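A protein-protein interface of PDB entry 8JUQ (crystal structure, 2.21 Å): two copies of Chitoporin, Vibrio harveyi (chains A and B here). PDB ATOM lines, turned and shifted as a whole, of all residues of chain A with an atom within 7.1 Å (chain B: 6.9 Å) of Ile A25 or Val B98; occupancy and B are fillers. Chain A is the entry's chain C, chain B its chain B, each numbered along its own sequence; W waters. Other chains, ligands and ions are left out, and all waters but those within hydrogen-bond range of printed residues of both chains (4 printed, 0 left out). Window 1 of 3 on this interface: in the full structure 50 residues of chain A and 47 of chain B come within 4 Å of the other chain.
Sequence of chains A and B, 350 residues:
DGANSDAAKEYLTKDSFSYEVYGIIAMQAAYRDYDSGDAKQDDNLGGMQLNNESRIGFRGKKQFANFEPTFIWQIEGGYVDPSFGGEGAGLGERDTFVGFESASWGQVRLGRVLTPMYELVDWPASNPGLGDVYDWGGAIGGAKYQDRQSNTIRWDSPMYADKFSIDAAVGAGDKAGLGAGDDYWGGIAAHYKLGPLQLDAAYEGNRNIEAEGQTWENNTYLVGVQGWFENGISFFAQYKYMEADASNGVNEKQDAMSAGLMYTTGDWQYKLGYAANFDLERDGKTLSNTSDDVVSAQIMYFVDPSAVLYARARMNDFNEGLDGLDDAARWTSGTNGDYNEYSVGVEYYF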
ATOM      1  N   GLY A  23     -13.555  12.117  15.019  1.00  0.00           N
ATOM      2  CA  GLY A  23     -12.303  12.818  14.841  1.00  0.00           C
ATOM      3  C   GLY A  23     -11.710  13.247  16.156  1.00  0.00           C
ATOM      4  O   GLY A  23     -12.409  13.430  17.156  1.00  0.00           O
ATOM      5  N   ILE A  24     -10.407  13.384  16.155  1.00  0.00           N
ATOM      6  CA  ILE A  24      -9.717  14.056  17.229  1.00  0.00           C
ATOM      7  C   ILE A  24      -9.101  15.302  16.618  1.00  0.00           C
ATOM      8  O   ILE A  24      -8.324  15.214  15.658  1.00  0.00           O
ATOM      9  CB  ILE A  24      -8.682  13.148  17.908  1.00  0.00           C
ATOM     10  CG1 ILE A  24      -9.409  12.039  18.675  1.00  0.00           C
ATOM     11  CG2 ILE A  24      -7.812  13.936  18.884  1.00  0.00           C
ATOM     12  CD1 ILE A  24      -9.788  10.862  17.792  1.00  0.00           C
ATOM     13  N   ILE A  25      -9.518  16.454  17.126  1.00  0.00           N
ATOM     14  CA  ILE A  25      -8.927  17.726  16.767  1.00  0.00           C
ATOM     15  C   ILE A  25      -7.831  17.984  17.790  1.00  0.00           C
ATOM     16  O   ILE A  25      -8.098  18.049  18.990  1.00  0.00           O
ATOM     17  CB  ILE A  25      -9.988  18.845  16.765  1.00  0.00           C
ATOM     18  CG1 ILE A  25     -11.183  18.465  15.876  1.00  0.00           C
ATOM     19  CG2 ILE A  25      -9.429  20.115  16.245  1.00  0.00           C
ATOM     20  CD1 ILE A  25     -10.793  17.915  14.508  1.00  0.00           C
ATOM     21  N   ALA A  26      -6.593  18.111  17.333  1.00  0.00           N
ATOM     22  CA  ALA A  26      -5.456  18.169  18.247  1.00  0.00           C
ATOM     23  C   ALA A  26      -4.433  19.124  17.662  1.00  0.00           C
ATOM     24  O   ALA A  26      -3.934  18.882  16.563  1.00  0.00           O
ATOM     25  CB  ALA A  26      -4.835  16.784  18.446  1.00  0.00           C
ATOM     26  N   MET A  27      -4.132  20.203  18.377  1.00  0.00           N
ATOM     27  CA  MET A  27      -3.180  21.196  17.904  1.00  0.00           C
ATOM     28  C   MET A  27      -2.244  21.508  19.059  1.00  0.00           C
ATOM     29  O   MET A  27      -2.696  21.752  20.180  1.00  0.00           O
ATOM     30  CB  MET A  27      -3.869  22.495  17.450  1.00  0.00           C
ATOM     31  CG  MET A  27      -2.927  23.605  16.934  1.00  0.00           C
ATOM     32  SD  MET A  27      -1.820  23.117  15.581  1.00  0.00           S
ATOM     33  CE  MET A  27      -2.907  23.478  14.188  1.00  0.00           C
ATOM     34  N   GLN A  28      -0.955  21.502  18.772  1.00  0.00           N
ATOM     35  CA  GLN A  28       0.079  21.836  19.726  1.00  0.00           C
ATOM     36  C   GLN A  28       0.988  22.887  19.106  1.00  0.00           C
ATOM     37  O   GLN A  28       1.608  22.641  18.060  1.00  0.00           O
ATOM     38  CB  GLN A  28       0.879  20.590  20.102  1.00  0.00           C
ATOM     39  CG  GLN A  28       2.026  20.814  21.054  1.00  0.00           C
ATOM     40  CD  GLN A  28       2.832  19.543  21.212  1.00  0.00           C
ATOM     41  OE1 GLN A  28       3.034  18.829  20.224  1.00  0.00           O
ATOM     42  NE2 GLN A  28       3.271  19.229  22.444  1.00  0.00           N
ATOM     43  N   ASN A  52       0.054  19.809  14.265  1.00  0.00           N
ATOM     44  CA  ASN A  52      -1.373  19.547  14.070  1.00  0.00           C
ATOM     45  C   ASN A  52      -1.562  18.042  13.937  1.00  0.00           C
ATOM     46  O   ASN A  52      -1.299  17.451  12.875  1.00  0.00           O
ATOM     47  CB  ASN A  52      -1.922  20.300  12.856  1.00  0.00           C
ATOM     48  CG  ASN A  52      -3.456  20.224  12.768  1.00  0.00           C
ATOM     49  OD1 ASN A  52      -4.087  19.459  13.492  1.00  0.00           O
ATOM     50  ND2 ASN A  52      -4.047  21.018  11.878  1.00  0.00           N
ATOM     51  N   GLU A  53      -2.013  17.413  15.020  1.00  0.00           N
ATOM     52  CA  GLU A  53      -2.241  15.975  15.044  1.00  0.00           C
ATOM     53  C   GLU A  53      -3.716  15.633  14.876  1.00  0.00           C
ATOM     54  O   GLU A  53      -4.144  14.540  15.271  1.00  0.00           O
ATOM     55  CB  GLU A  53      -1.679  15.370  16.336  1.00  0.00           C
ATOM     56  CG  GLU A  53      -0.148  15.554  16.447  1.00  0.00           C
ATOM     57  CD  GLU A  53       0.490  14.975  17.726  1.00  0.00           C
ATOM     58  OE1 GLU A  53      -0.130  15.054  18.816  1.00  0.00           O
ATOM     59  OE2 GLU A  53       1.667  14.515  17.664  1.00  0.00           O
ATOM     60  N   SER A  54      -4.503  16.563  14.319  1.00  0.00           N
ATOM     61  CA  SER A  54      -5.891  16.272  14.000  1.00  0.00           C
ATOM     62  C   SER A  54      -5.989  15.100  13.019  1.00  0.00           C
ATOM     63  O   SER A  54      -5.159  14.950  12.116  1.00  0.00           O
ATOM     64  CB  SER A  54      -6.572  17.516  13.413  1.00  0.00           C
ATOM     65  OG  SER A  54      -6.524  18.602  14.330  1.00  0.00           O
ATOM     66  N   ARG A  55      -7.024  14.279  13.191  1.00  0.00           N
ATOM     67  CA  ARG A  55      -7.280  13.179  12.278  1.00  0.00           C
ATOM     68  C   ARG A  55      -8.768  12.877  12.251  1.00  0.00           C
ATOM     69  O   ARG A  55      -9.489  13.094  13.232  1.00  0.00           O
ATOM     70  CB  ARG A  55      -6.494  11.909  12.644  1.00  0.00           C
ATOM     71  CG  ARG A  55      -6.832  11.295  13.992  1.00  0.00           C
ATOM     72  CD  ARG A  55      -5.926  11.859  15.023  1.00  0.00           C
ATOM     73  NE  ARG A  55      -5.886  11.118  16.274  1.00  0.00           N
ATOM     74  CZ  ARG A  55      -5.301  11.574  17.371  1.00  0.00           C
ATOM     75  NH1 ARG A  55      -4.746  12.781  17.405  1.00  0.00           N
ATOM     76  NH2 ARG A  55      -5.304  10.821  18.472  1.00  0.00           N
ATOM     77  N   ILE A  56      -9.208  12.380  11.101  1.00  0.00           N
ATOM     78  CA  ILE A  56     -10.579  11.982  10.837  1.00  0.00           C
ATOM     79  C   ILE A  56     -10.608  10.463  10.716  1.00  0.00           C
ATOM     80  O   ILE A  56      -9.670   9.862  10.182  1.00  0.00           O
ATOM     81  CB  ILE A  56     -11.088  12.667   9.551  1.00  0.00           C
ATOM     82  CG1 ILE A  56     -11.155  14.191   9.761  1.00  0.00           C
ATOM     83  CG2 ILE A  56     -12.467  12.145   9.167  1.00  0.00           C
ATOM     84  CD1 ILE A  56     -12.269  14.590  10.746  1.00  0.00           C
ATOM     85  N   SER A 306     -15.479  17.175  26.477  1.00  0.00           N
ATOM     86  CA  SER A 306     -14.928  16.677  25.224  1.00  0.00           C
ATOM     87  C   SER A 306     -13.543  17.196  24.893  1.00  0.00           C
ATOM     88  O   SER A 306     -13.005  16.816  23.847  1.00  0.00           O
ATOM     89  CB  SER A 306     -15.859  17.058  24.070  1.00  0.00           C
ATOM     90  OG  SER A 306     -16.988  16.232  24.073  1.00  0.00           O
ATOM     91  N   VAL A 308      -9.622  19.300  26.274  1.00  0.00           N
ATOM     92  CA  VAL A 308      -8.664  19.775  27.262  1.00  0.00           C
ATOM     93  C   VAL A 308      -7.808  20.850  26.624  1.00  0.00           C
ATOM     94  O   VAL A 308      -7.589  20.846  25.411  1.00  0.00           O
ATOM     95  CB  VAL A 308      -7.764  18.641  27.800  1.00  0.00           C
ATOM     96  CG1 VAL A 308      -8.599  17.599  28.560  1.00  0.00           C
ATOM     97  CG2 VAL A 308      -6.990  17.995  26.663  1.00  0.00           C
ATOM     98  N   VAL A 346      -4.374  21.930  22.474  1.00  0.00           N
ATOM     99  CA  VAL A 346      -5.779  21.606  22.677  1.00  0.00           C
ATOM    100  C   VAL A 346      -6.038  20.220  22.094  1.00  0.00           C
ATOM    101  O   VAL A 346      -5.414  19.824  21.112  1.00  0.00           O
ATOM    102  CB  VAL A 346      -6.696  22.679  22.039  1.00  0.00           C
ATOM    103  CG1 VAL A 346      -6.409  22.808  20.566  1.00  0.00           C
ATOM    104  CG2 VAL A 346      -8.180  22.353  22.294  1.00  0.00           C
ATOM    105  N   GLU A 347      -6.929  19.458  22.726  1.00  0.00           N
ATOM    106  CA  GLU A 347      -7.404  18.216  22.123  1.00  0.00           C
ATOM    107  C   GLU A 347      -8.910  18.139  22.311  1.00  0.00           C
ATOM    108  O   GLU A 347      -9.425  18.464  23.391  1.00  0.00           O
ATOM    109  CB  GLU A 347      -6.779  16.976  22.749  1.00  0.00           C
ATOM    110  CG  GLU A 347      -5.251  17.050  22.673  1.00  0.00           C
ATOM    111  CD  GLU A 347      -4.567  15.791  22.149  1.00  0.00           C
ATOM    112  OE1 GLU A 347      -5.274  14.805  21.768  1.00  0.00           O
ATOM    113  OE2 GLU A 347      -3.309  15.823  22.103  1.00  0.00           O
ATOM    114  N   TYR A 348      -9.610  17.702  21.262  1.00  0.00           N
ATOM    115  CA  TYR A 348     -11.069  17.684  21.260  1.00  0.00           C
ATOM    116  C   TYR A 348     -11.543  16.460  20.493  1.00  0.00           C
ATOM    117  O   TYR A 348     -11.066  16.200  19.377  1.00  0.00           O
ATOM    118  CB  TYR A 348     -11.618  18.973  20.630  1.00  0.00           C
ATOM    119  CG  TYR A 348     -13.059  18.960  20.237  1.00  0.00           C
ATOM    120  CD1 TYR A 348     -14.061  18.855  21.194  1.00  0.00           C
ATOM    121  CD2 TYR A 348     -13.436  19.125  18.896  1.00  0.00           C
ATOM    122  CE1 TYR A 348     -15.401  18.877  20.824  1.00  0.00           C
ATOM    123  CE2 TYR A 348     -14.762  19.152  18.519  1.00  0.00           C
ATOM    124  CZ  TYR A 348     -15.741  19.021  19.490  1.00  0.00           C
ATOM    125  OH  TYR A 348     -17.069  19.027  19.118  1.00  0.00           O
ATOM    126  N   TYR A 349     -12.520  15.752  21.061  1.00  0.00           N
ATOM    127  CA  TYR A 349     -13.000  14.481  20.521  1.00  0.00           C
ATOM    128  C   TYR A 349     -14.463  14.614  20.090  1.00  0.00           C
ATOM    129  O   TYR A 349     -15.340  14.909  20.915  1.00  0.00           O
ATOM    130  CB  TYR A 349     -12.832  13.384  21.578  1.00  0.00           C
ATOM    131  CG  TYR A 349     -13.216  11.993  21.178  1.00  0.00           C
ATOM    132  CD1 TYR A 349     -13.131  11.577  19.851  1.00  0.00           C
ATOM    133  CD2 TYR A 349     -13.631  11.068  22.142  1.00  0.00           C
ATOM    134  CE1 TYR A 349     -13.461  10.292  19.497  1.00  0.00           C
ATOM    135  CE2 TYR A 349     -13.954   9.755  21.796  1.00  0.00           C
ATOM    136  CZ  TYR A 349     -13.874   9.379  20.474  1.00  0.00           C
ATOM    137  OH  TYR A 349     -14.210   8.099  20.095  1.00  0.00           O
ATOM    138  N   PHE A 350     -14.732  14.397  18.806  1.00  0.00           N
ATOM    139  CA  PHE A 350     -16.129  14.322  18.357  1.00  0.00           C
ATOM    140  C   PHE A 350     -16.429  12.988  17.664  1.00  0.00           C
ATOM    141  O   PHE A 350     -17.618  12.650  17.539  1.00  0.00           O
ATOM    142  CB  PHE A 350     -16.474  15.474  17.411  1.00  0.00           C
ATOM    143  CG  PHE A 350     -15.879  15.324  16.041  1.00  0.00           C
ATOM    144  CD1 PHE A 350     -16.571  14.650  15.035  1.00  0.00           C
ATOM    145  CD2 PHE A 350     -14.623  15.862  15.755  1.00  0.00           C
ATOM    146  CE1 PHE A 350     -16.010  14.494  13.771  1.00  0.00           C
ATOM    147  CE2 PHE A 350     -14.058  15.723  14.474  1.00  0.00           C
ATOM    148  CZ  PHE A 350     -14.758  15.043  13.488  1.00  0.00           C
ATOM    149  OXT PHE A 350     -15.530  12.251  17.192  1.00  0.00           O
ATOM    150  N   ALA B   8      -7.313  11.090  24.304  1.00  0.00           N
ATOM    151  CA  ALA B   8      -8.574  11.783  24.076  1.00  0.00           C
ATOM    152  C   ALA B   8      -9.696  10.784  23.811  1.00  0.00           C
ATOM    153  O   ALA B   8     -10.789  10.892  24.379  1.00  0.00           O
ATOM    154  CB  ALA B   8      -8.424  12.780  22.928  1.00  0.00           C
ATOM    155  N   PHE B  71     -14.806  27.619  19.996  1.00  0.00           N
ATOM    156  CA  PHE B  71     -13.749  26.857  19.342  1.00  0.00           C
ATOM    157  C   PHE B  71     -14.194  26.513  17.928  1.00  0.00           C
ATOM    158  O   PHE B  71     -15.331  26.079  17.719  1.00  0.00           O
ATOM    159  CB  PHE B  71     -13.440  25.583  20.155  1.00  0.00           C
ATOM    160  CG  PHE B  71     -12.376  24.674  19.546  1.00  0.00           C
ATOM    161  CD1 PHE B  71     -11.045  25.005  19.606  1.00  0.00           C
ATOM    162  CD2 PHE B  71     -12.726  23.462  18.988  1.00  0.00           C
ATOM    163  CE1 PHE B  71     -10.073  24.177  19.097  1.00  0.00           C
ATOM    164  CE2 PHE B  71     -11.771  22.605  18.487  1.00  0.00           C
ATOM    165  CZ  PHE B  71     -10.425  22.972  18.536  1.00  0.00           C
ATOM    166  N   ILE B  72     -13.306  26.713  16.958  1.00  0.00           N
ATOM    167  CA  ILE B  72     -13.586  26.400  15.563  1.00  0.00           C
ATOM    168  C   ILE B  72     -12.453  25.530  15.055  1.00  0.00           C
ATOM    169  O   ILE B  72     -11.320  25.620  15.530  1.00  0.00           O
ATOM    170  CB  ILE B  72     -13.725  27.656  14.676  1.00  0.00           C
ATOM    171  CG1 ILE B  72     -12.368  28.383  14.593  1.00  0.00           C
ATOM    172  CG2 ILE B  72     -14.815  28.590  15.221  1.00  0.00           C
ATOM    173  CD1 ILE B  72     -12.370  29.564  13.623  1.00  0.00           C
ATOM    174  N   TRP B  73     -12.777  24.661  14.103  1.00  0.00           N
ATOM    175  CA  TRP B  73     -11.776  23.806  13.487  1.00  0.00           C
ATOM    176  C   TRP B  73     -12.217  23.488  12.067  1.00  0.00           C
ATOM    177  O   TRP B  73     -13.410  23.457  11.750  1.00  0.00           O
ATOM    178  CB  TRP B  73     -11.562  22.486  14.264  1.00  0.00           C
ATOM    179  CG  TRP B  73     -12.806  21.643  14.335  1.00  0.00           C
ATOM    180  CD1 TRP B  73     -13.785  21.718  15.290  1.00  0.00           C
ATOM    181  CD2 TRP B  73     -13.236  20.642  13.396  1.00  0.00           C
ATOM    182  NE1 TRP B  73     -14.772  20.814  15.015  1.00  0.00           N
ATOM    183  CE2 TRP B  73     -14.461  20.136  13.863  1.00  0.00           C
ATOM    184  CE3 TRP B  73     -12.680  20.092  12.238  1.00  0.00           C
ATOM    185  CZ2 TRP B  73     -15.171  19.137  13.183  1.00  0.00           C
ATOM    186  CZ3 TRP B  73     -13.374  19.092  11.575  1.00  0.00           C
ATOM    187  CH2 TRP B  73     -14.607  18.624  12.049  1.00  0.00           C
ATOM    188  N   GLN B  74     -11.227  23.172  11.237  1.00  0.00           N
ATOM    189  CA  GLN B  74     -11.474  22.797   9.860  1.00  0.00           C
ATOM    190  C   GLN B  74     -10.357  21.875   9.386  1.00  0.00           C
ATOM    191  O   GLN B  74      -9.182  22.100   9.715  1.00  0.00           O
ATOM    192  CB  GLN B  74     -11.544  24.043   8.966  1.00  0.00           C
ATOM    193  CG  GLN B  74     -11.705  23.689   7.507  1.00  0.00           C
ATOM    194  CD  GLN B  74     -12.027  24.905   6.660  1.00  0.00           C
ATOM    195  OE1 GLN B  74     -13.115  25.477   6.768  1.00  0.00           O
ATOM    196  NE2 GLN B  74     -11.067  25.322   5.829  1.00  0.00           N
ATOM    197  N   ILE B  75     -10.724  20.853   8.602  1.00  0.00           N
ATOM    198  CA  ILE B  75      -9.770  19.981   7.910  1.00  0.00           C
ATOM    199  C   ILE B  75     -10.256  19.843   6.477  1.00  0.00           C
ATOM    200  O   ILE B  75     -11.310  19.250   6.245  1.00  0.00           O
ATOM    201  CB  ILE B  75      -9.670  18.598   8.565  1.00  0.00           C
ATOM    202  CG1 ILE B  75      -9.288  18.719  10.037  1.00  0.00           C
ATOM    203  CG2 ILE B  75      -8.697  17.677   7.775  1.00  0.00           C
ATOM    204  CD1 ILE B  75      -9.313  17.340  10.752  1.00  0.00           C
ATOM    205  N   THR B  96      -6.644  24.146   6.997  1.00  0.00           N
ATOM    206  CA  THR B  96      -6.767  23.141   8.044  1.00  0.00           C
ATOM    207  C   THR B  96      -6.276  23.795   9.329  1.00  0.00           C
ATOM    208  O   THR B  96      -5.094  24.133   9.411  1.00  0.00           O
ATOM    209  CB  THR B  96      -5.919  21.909   7.681  1.00  0.00           C
ATOM    210  OG1 THR B  96      -6.457  21.318   6.501  1.00  0.00           O
ATOM    211  CG2 THR B  96      -5.896  20.898   8.776  1.00  0.00           C
ATOM    212  N   PHE B  97      -7.154  24.000  10.317  1.00  0.00           N
ATOM    213  CA  PHE B  97      -6.770  24.861  11.432  1.00  0.00           C
ATOM    214  C   PHE B  97      -7.662  24.572  12.625  1.00  0.00           C
ATOM    215  O   PHE B  97      -8.703  23.924  12.502  1.00  0.00           O
ATOM    216  CB  PHE B  97      -6.864  26.352  11.050  1.00  0.00           C
ATOM    217  CG  PHE B  97      -8.225  26.755  10.565  1.00  0.00           C
ATOM    218  CD1 PHE B  97      -9.260  26.983  11.460  1.00  0.00           C
ATOM    219  CD2 PHE B  97      -8.490  26.824   9.209  1.00  0.00           C
ATOM    220  CE1 PHE B  97     -10.539  27.287  10.996  1.00  0.00           C
ATOM    221  CE2 PHE B  97      -9.748  27.178   8.740  1.00  0.00           C
ATOM    222  CZ  PHE B  97     -10.768  27.413   9.624  1.00  0.00           C
ATOM    223  N   VAL B  98      -7.213  25.049  13.793  1.00  0.00           N
ATOM    224  CA  VAL B  98      -8.052  25.234  14.967  1.00  0.00           C
ATOM    225  C   VAL B  98      -8.045  26.722  15.296  1.00  0.00           C
ATOM    226  O   VAL B  98      -7.170  27.480  14.864  1.00  0.00           O
ATOM    227  CB  VAL B  98      -7.567  24.407  16.195  1.00  0.00           C
ATOM    228  CG1 VAL B  98      -7.428  22.946  15.837  1.00  0.00           C
ATOM    229  CG2 VAL B  98      -6.262  24.973  16.730  1.00  0.00           C
ATOM    230  N   GLY B  99      -9.018  27.137  16.086  1.00  0.00           N
ATOM    231  CA  GLY B  99      -9.042  28.532  16.477  1.00  0.00           C
ATOM    232  C   GLY B  99     -10.166  28.813  17.444  1.00  0.00           C
ATOM    233  O   GLY B  99     -10.878  27.909  17.901  1.00  0.00           O
ATOM    234  N   PHE B 100     -10.293  30.096  17.765  1.00  0.00           N
ATOM    235  CA  PHE B 100     -11.332  30.613  18.644  1.00  0.00           C
ATOM    236  C   PHE B 100     -11.908  31.877  18.030  1.00  0.00           C
ATOM    237  O   PHE B 100     -11.203  32.594  17.323  1.00  0.00           O
ATOM    238  CB  PHE B 100     -10.788  30.943  20.046  1.00  0.00           C
ATOM    239  CG  PHE B 100     -10.403  29.741  20.829  1.00  0.00           C
ATOM    240  CD1 PHE B 100     -11.365  29.009  21.500  1.00  0.00           C
ATOM    241  CD2 PHE B 100      -9.102  29.322  20.867  1.00  0.00           C
ATOM    242  CE1 PHE B 100     -11.034  27.890  22.212  1.00  0.00           C
ATOM    243  CE2 PHE B 100      -8.750  28.196  21.589  1.00  0.00           C
ATOM    244  CZ  PHE B 100      -9.724  27.479  22.259  1.00  0.00           C
ATOM    245  N   VAL B 108      -9.095  34.047  15.823  1.00  0.00           N
ATOM    246  CA  VAL B 108      -7.695  33.668  15.749  1.00  0.00           C
ATOM    247  C   VAL B 108      -7.665  32.214  15.325  1.00  0.00           C
ATOM    248  O   VAL B 108      -8.391  31.398  15.892  1.00  0.00           O
ATOM    249  CB  VAL B 108      -6.953  33.885  17.087  1.00  0.00           C
ATOM    250  CG1 VAL B 108      -7.607  33.097  18.212  1.00  0.00           C
ATOM    251  CG2 VAL B 108      -5.483  33.461  16.965  1.00  0.00           C
ATOM    252  N   ARG B 109      -6.844  31.901  14.313  1.00  0.00           N
ATOM    253  CA  ARG B 109      -6.691  30.557  13.778  1.00  0.00           C
ATOM    254  C   ARG B 109      -5.220  30.162  13.822  1.00  0.00           C
ATOM    255  O   ARG B 109      -4.324  31.006  13.644  1.00  0.00           O
ATOM    256  CB  ARG B 109      -7.210  30.429  12.320  1.00  0.00           C
ATOM    257  CG  ARG B 109      -8.730  30.499  12.171  1.00  0.00           C
ATOM    258  CD  ARG B 109      -9.170  30.468  10.693  1.00  0.00           C
ATOM    259  NE  ARG B 109      -8.870  31.716   9.998  1.00  0.00           N
ATOM    260  CZ  ARG B 109      -8.800  31.858   8.677  1.00  0.00           C
ATOM    261  NH1 ARG B 109      -8.986  30.832   7.860  1.00  0.00           N
ATOM    262  NH2 ARG B 109      -8.516  33.059   8.160  1.00  0.00           N
ATOM    263  N   LEU B 110      -4.984  28.890  14.120  1.00  0.00           N
ATOM    264  CA  LEU B 110      -3.662  28.293  14.131  1.00  0.00           C
ATOM    265  C   LEU B 110      -3.683  27.116  13.176  1.00  0.00           C
ATOM    266  O   LEU B 110      -4.556  26.250  13.272  1.00  0.00           O
ATOM    267  CB  LEU B 110      -3.255  27.813  15.532  1.00  0.00           C
ATOM    268  CG  LEU B 110      -2.981  28.858  16.606  1.00  0.00           C
ATOM    269  CD1 LEU B 110      -4.281  29.484  17.070  1.00  0.00           C
ATOM    270  CD2 LEU B 110      -2.307  28.185  17.779  1.00  0.00           C
ATOM    271  N   GLY B 111      -2.716  27.070  12.278  1.00  0.00           N
ATOM    272  CA  GLY B 111      -2.627  25.935  11.390  1.00  0.00           C
ATOM    273  C   GLY B 111      -2.182  26.357  10.018  1.00  0.00           C
ATOM    274  O   GLY B 111      -1.194  27.081   9.868  1.00  0.00           O
ATOM    275  N   ARG B 112      -2.941  25.941   9.019  1.00  0.00           N
ATOM    276  CA  ARG B 112      -2.586  26.104   7.614  1.00  0.00           C
ATOM    277  C   ARG B 112      -3.662  26.962   6.967  1.00  0.00           C
ATOM    278  O   ARG B 112      -4.789  26.498   6.764  1.00  0.00           O
ATOM    279  CB  ARG B 112      -2.465  24.730   6.940  1.00  0.00           C
ATOM    280  CG  ARG B 112      -2.126  24.769   5.449  1.00  0.00           C
ATOM    281  CD  ARG B 112      -1.926  23.329   4.881  1.00  0.00           C
ATOM    282  NE  ARG B 112      -1.707  23.365   3.436  1.00  0.00           N
ATOM    283  CZ  ARG B 112      -0.586  23.813   2.886  1.00  0.00           C
ATOM    284  NH1 ARG B 112       0.440  24.196   3.631  1.00  0.00           N
ATOM    285  NH2 ARG B 112      -0.510  23.929   1.563  1.00  0.00           N
HETATM  286  O   HOH W   1     -17.405  20.398  16.386  1.00  0.00           O
HETATM  287  O   HOH W   2      -5.310  11.848  22.129  1.00  0.00           O
HETATM  288  O   HOH W   3      -2.762  22.680  10.135  1.00  0.00           O
HETATM  289  O   HOH W   4      -7.071  20.915  11.998  1.00  0.00           O
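Water W3 lies within hydrogen-bond range of the side-chain amide nitrogen of Asn A52 (2.7 Å), the backbone carbonyl oxygen of Thr B96 (2.8 Å) and the backbone NH of Arg B112 (3.5 Å). Water W2 bridges the side-chain carboxylate (OE1) of Glu A347 (3.0 Å) and the backbone NH (N) of Ala B8 (3.1 Å). Water W1 lies within hydrogen-bond range of the indole nitrogen of Trp B73 (3.0 Å) and the side-chain hydroxyl of Tyr A348 (3.1 Å). Water W4 lies within hydrogen-bond range of ND2 of Asn A52 (3.0 Å), O of Gln B74 (3.3 Å), OG of Ser A54 (3.3 Å) and O of Phe B97 (3.5 Å).
No position is printed for both chains.
Among the printed residues, pairs that only touch across the chains: Met A27 with Leu B110 (3.4 Å), Ile A25 with Val B98 (3.5 Å), Met A27 with Val B98 (3.5 Å), Asn A52 with Thr B96 (3.6 Å), Tyr A349 with Ala B8 (3.6 Å), Ile A25 with Trp B73 (3.7 Å), Met A27 with Gly B111 (3.7 Å), Ile A56 with Ile B75 (3.8 Å), Ile A25 with Phe B71 (3.8 Å), Phe A350 with Trp B73 (3.8 Å), Ser A54 with Ile B75 (3.8 Å), Tyr A348 with Trp B73 (3.9 Å), Tyr A348 with Phe B71 (3.9 Å) and Glu A347 with Ala B8 (3.9 Å).
The backbone carbonyl oxygen (O) of Thr B96 is in hydrogen-bond range of the backbone NH (N) of Arg B112. O of Ala A26 lies close to OD1 of Asn A52, 3.1 Å away. The backbone NH (N) of Ala A26 is in hydrogen-bond range of the side-chain hydroxyl (OG) of Ser A54, at 3.0 Å. The backbone carbonyl oxygen (O) of Met A27 is in hydrogen-bond range of the backbone NH (N) of Val A346. The side-chain hydroxyl (OG) of Ser A54 lies within hydrogen-bond range of the side-chain amide oxygen (OD1) of Asn A52, at 2.7 Å. N of Tyr A349 lies within hydrogen-bond range of O of Ser A306.
Printed residues of chain B within 4 Å of Ile A25: Phe B71 (3.8 Å), Trp B73 (3.7 Å) and Val B98 (3.5 Å). Of the printed residues of chain B, Ser A54 touches Ile B75. Of the printed residues of chain B, Tyr A348 touches Phe B71 and Trp B73. Arg B109 touches none of the printed residues of chain A. The nearest printed residue of chain B that does not touch Asn A52 is Phe B97 (4.6 Å).
Of the 18 printed residues of chain A, 9 touch a printed residue of chain B. Hydrophobic or aromatic side chains of chain B within 4 Å of the printed part of chain A: Ala B8, Phe B71, Trp B73, Ile B75 and Val B98. Among the printed residues, 14 pairs touch across the chains.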
